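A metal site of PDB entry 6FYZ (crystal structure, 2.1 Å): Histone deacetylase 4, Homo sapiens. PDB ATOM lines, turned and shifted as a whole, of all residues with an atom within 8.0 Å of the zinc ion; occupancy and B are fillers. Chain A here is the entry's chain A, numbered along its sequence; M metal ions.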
ATOM      1  N   GLN A  22      15.537 -19.639   8.111  1.00  0.00           N
ATOM      2  CA  GLN A  22      15.093 -20.375   6.921  1.00  0.00           C
ATOM      3  C   GLN A  22      15.466 -21.828   7.131  1.00  0.00           C
ATOM      4  O   GLN A  22      16.538 -22.141   7.652  1.00  0.00           O
ATOM      5  CB  GLN A  22      15.798 -19.794   5.677  1.00  0.00           C
ATOM      6  CG  GLN A  22      15.327 -20.298   4.319  1.00  0.00           C
ATOM      7  CD  GLN A  22      14.087 -19.576   3.790  1.00  0.00           C
ATOM      8  OE1 GLN A  22      13.222 -19.119   4.564  1.00  0.00           O
ATOM      9  NE2 GLN A  22      13.978 -19.486   2.462  1.00  0.00           N
ATOM     10  N   CYS A  23      14.564 -22.728   6.744  1.00  0.00           N
ATOM     11  CA  CYS A  23      14.888 -24.153   6.741  1.00  0.00           C
ATOM     12  C   CYS A  23      15.963 -24.436   5.693  1.00  0.00           C
ATOM     13  O   CYS A  23      15.988 -23.800   4.638  1.00  0.00           O
ATOM     14  CB  CYS A  23      13.674 -25.009   6.468  1.00  0.00           C
ATOM     15  SG  CYS A  23      13.914 -26.691   7.072  1.00  0.00           S
ATOM     16  N   THR A  24      16.820 -25.407   5.997  1.00  0.00           N
ATOM     17  CA  THR A  24      17.947 -25.749   5.116  1.00  0.00           C
ATOM     18  C   THR A  24      17.518 -26.337   3.758  1.00  0.00           C
ATOM     19  O   THR A  24      18.280 -26.247   2.793  1.00  0.00           O
ATOM     20  CB  THR A  24      18.928 -26.721   5.831  1.00  0.00           C
ATOM     21  OG1 THR A  24      18.201 -27.785   6.457  1.00  0.00           O
ATOM     22  CG2 THR A  24      19.733 -25.971   6.888  1.00  0.00           C
ATOM     23  N   CYS A  25      16.296 -26.892   3.674  1.00  0.00           N
ATOM     24  CA  CYS A  25      15.687 -27.290   2.391  1.00  0.00           C
ATOM     25  C   CYS A  25      15.466 -26.070   1.456  1.00  0.00           C
ATOM     26  O   CYS A  25      15.475 -26.228   0.235  1.00  0.00           O
ATOM     27  CB  CYS A  25      14.361 -28.042   2.599  1.00  0.00           C
ATOM     28  SG  CYS A  25      12.889 -27.003   2.930  1.00  0.00           S
ATOM     29  N   GLY A  26      15.243 -24.897   2.039  1.00  0.00           N
ATOM     30  CA  GLY A  26      15.153 -23.635   1.289  1.00  0.00           C
ATOM     31  C   GLY A  26      13.880 -23.394   0.497  1.00  0.00           C
ATOM     32  O   GLY A  26      13.851 -22.509  -0.359  1.00  0.00           O
ATOM     33  N   SER A  27      12.811 -24.160   0.789  1.00  0.00           N
ATOM     34  CA  SER A  27      11.558 -24.086   0.021  1.00  0.00           C
ATOM     35  C   SER A  27      10.548 -23.129   0.663  1.00  0.00           C
ATOM     36  O   SER A  27      10.347 -23.126   1.881  1.00  0.00           O
ATOM     37  CB  SER A  27      10.932 -25.478  -0.118  1.00  0.00           C
ATOM     38  OG  SER A  27      10.203 -25.860   1.035  1.00  0.00           O
ATOM     39  N   SER A  28       9.914 -22.312  -0.191  1.00  0.00           N
ATOM     40  CA  SER A  28       8.763 -21.490   0.202  1.00  0.00           C
ATOM     41  C   SER A  28       7.532 -22.363   0.441  1.00  0.00           C
ATOM     42  O   SER A  28       6.796 -22.144   1.407  1.00  0.00           O
ATOM     43  CB  SER A  28       8.440 -20.464  -0.895  1.00  0.00           C
ATOM     44  OG  SER A  28       9.604 -20.030  -1.567  1.00  0.00           O
ATOM     45  N   SER A  30       6.892 -25.526   1.459  1.00  0.00           N
ATOM     46  CA  SER A  30       6.740 -26.323   2.671  1.00  0.00           C
ATOM     47  C   SER A  30       6.729 -25.497   3.979  1.00  0.00           C
ATOM     48  O   SER A  30       6.410 -26.035   5.031  1.00  0.00           O
ATOM     49  CB  SER A  30       7.835 -27.407   2.723  1.00  0.00           C
ATOM     50  OG  SER A  30       7.338 -28.598   3.302  1.00  0.00           O
ATOM     51  N   HIS A  31       7.076 -24.210   3.901  1.00  0.00           N
ATOM     52  CA  HIS A  31       7.085 -23.312   5.077  1.00  0.00           C
ATOM     53  C   HIS A  31       6.620 -21.904   4.668  1.00  0.00           C
ATOM     54  O   HIS A  31       7.407 -21.120   4.119  1.00  0.00           O
ATOM     55  CB  HIS A  31       8.494 -23.261   5.692  1.00  0.00           C
ATOM     56  CG  HIS A  31       9.085 -24.612   5.957  1.00  0.00           C
ATOM     57  ND1 HIS A  31       8.600 -25.468   6.923  1.00  0.00           N
ATOM     58  CD2 HIS A  31      10.115 -25.268   5.367  1.00  0.00           C
ATOM     59  CE1 HIS A  31       9.315 -26.582   6.929  1.00  0.00           C
ATOM     60  NE2 HIS A  31      10.232 -26.489   5.984  1.00  0.00           N
ATOM     61  N   ILE A 117       9.728 -24.164  11.703  1.00  0.00           N
ATOM     62  CA  ILE A 117      11.133 -24.210  11.308  1.00  0.00           C
ATOM     63  C   ILE A 117      12.054 -23.657  12.381  1.00  0.00           C
ATOM     64  O   ILE A 117      11.714 -22.701  13.066  1.00  0.00           O
ATOM     65  CB  ILE A 117      11.392 -23.431   9.994  1.00  0.00           C
ATOM     66  CG1 ILE A 117      10.931 -21.956  10.104  1.00  0.00           C
ATOM     67  CG2 ILE A 117      10.700 -24.130   8.832  1.00  0.00           C
ATOM     68  CD1 ILE A 117      11.119 -21.129   8.836  1.00  0.00           C
ATOM     69  N   TRP A 118      13.217 -24.280  12.519  1.00  0.00           N
ATOM     70  CA  TRP A 118      14.266 -23.729  13.357  1.00  0.00           C
ATOM     71  C   TRP A 118      15.636 -23.967  12.729  1.00  0.00           C
ATOM     72  O   TRP A 118      16.090 -25.103  12.658  1.00  0.00           O
ATOM     73  CB  TRP A 118      14.221 -24.321  14.772  1.00  0.00           C
ATOM     74  CG  TRP A 118      15.077 -23.545  15.697  1.00  0.00           C
ATOM     75  CD1 TRP A 118      16.268 -23.934  16.240  1.00  0.00           C
ATOM     76  CD2 TRP A 118      14.839 -22.216  16.162  1.00  0.00           C
ATOM     77  NE1 TRP A 118      16.773 -22.938  17.030  1.00  0.00           N
ATOM     78  CE2 TRP A 118      15.913 -21.867  17.001  1.00  0.00           C
ATOM     79  CE3 TRP A 118      13.813 -21.280  15.955  1.00  0.00           C
ATOM     80  CZ2 TRP A 118      16.002 -20.624  17.639  1.00  0.00           C
ATOM     81  CZ3 TRP A 118      13.898 -20.044  16.578  1.00  0.00           C
ATOM     82  CH2 TRP A 118      14.982 -19.722  17.409  1.00  0.00           C
HETATM   83 ZN    ZN M   1      12.215 -27.438   5.446  1.00  0.00          ZN
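SG of Cys 25 sits close to OG of Ser 27 (3.5 Å).
The zinc ion is bound by NE2 of His 31, 2.3 Å away. SG of Cys 23 binds the zinc ion (2.5 Å). SG of Cys 25 binds the zinc ion, at 2.6 Å. The zinc ion has three donor atoms within binding distance.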
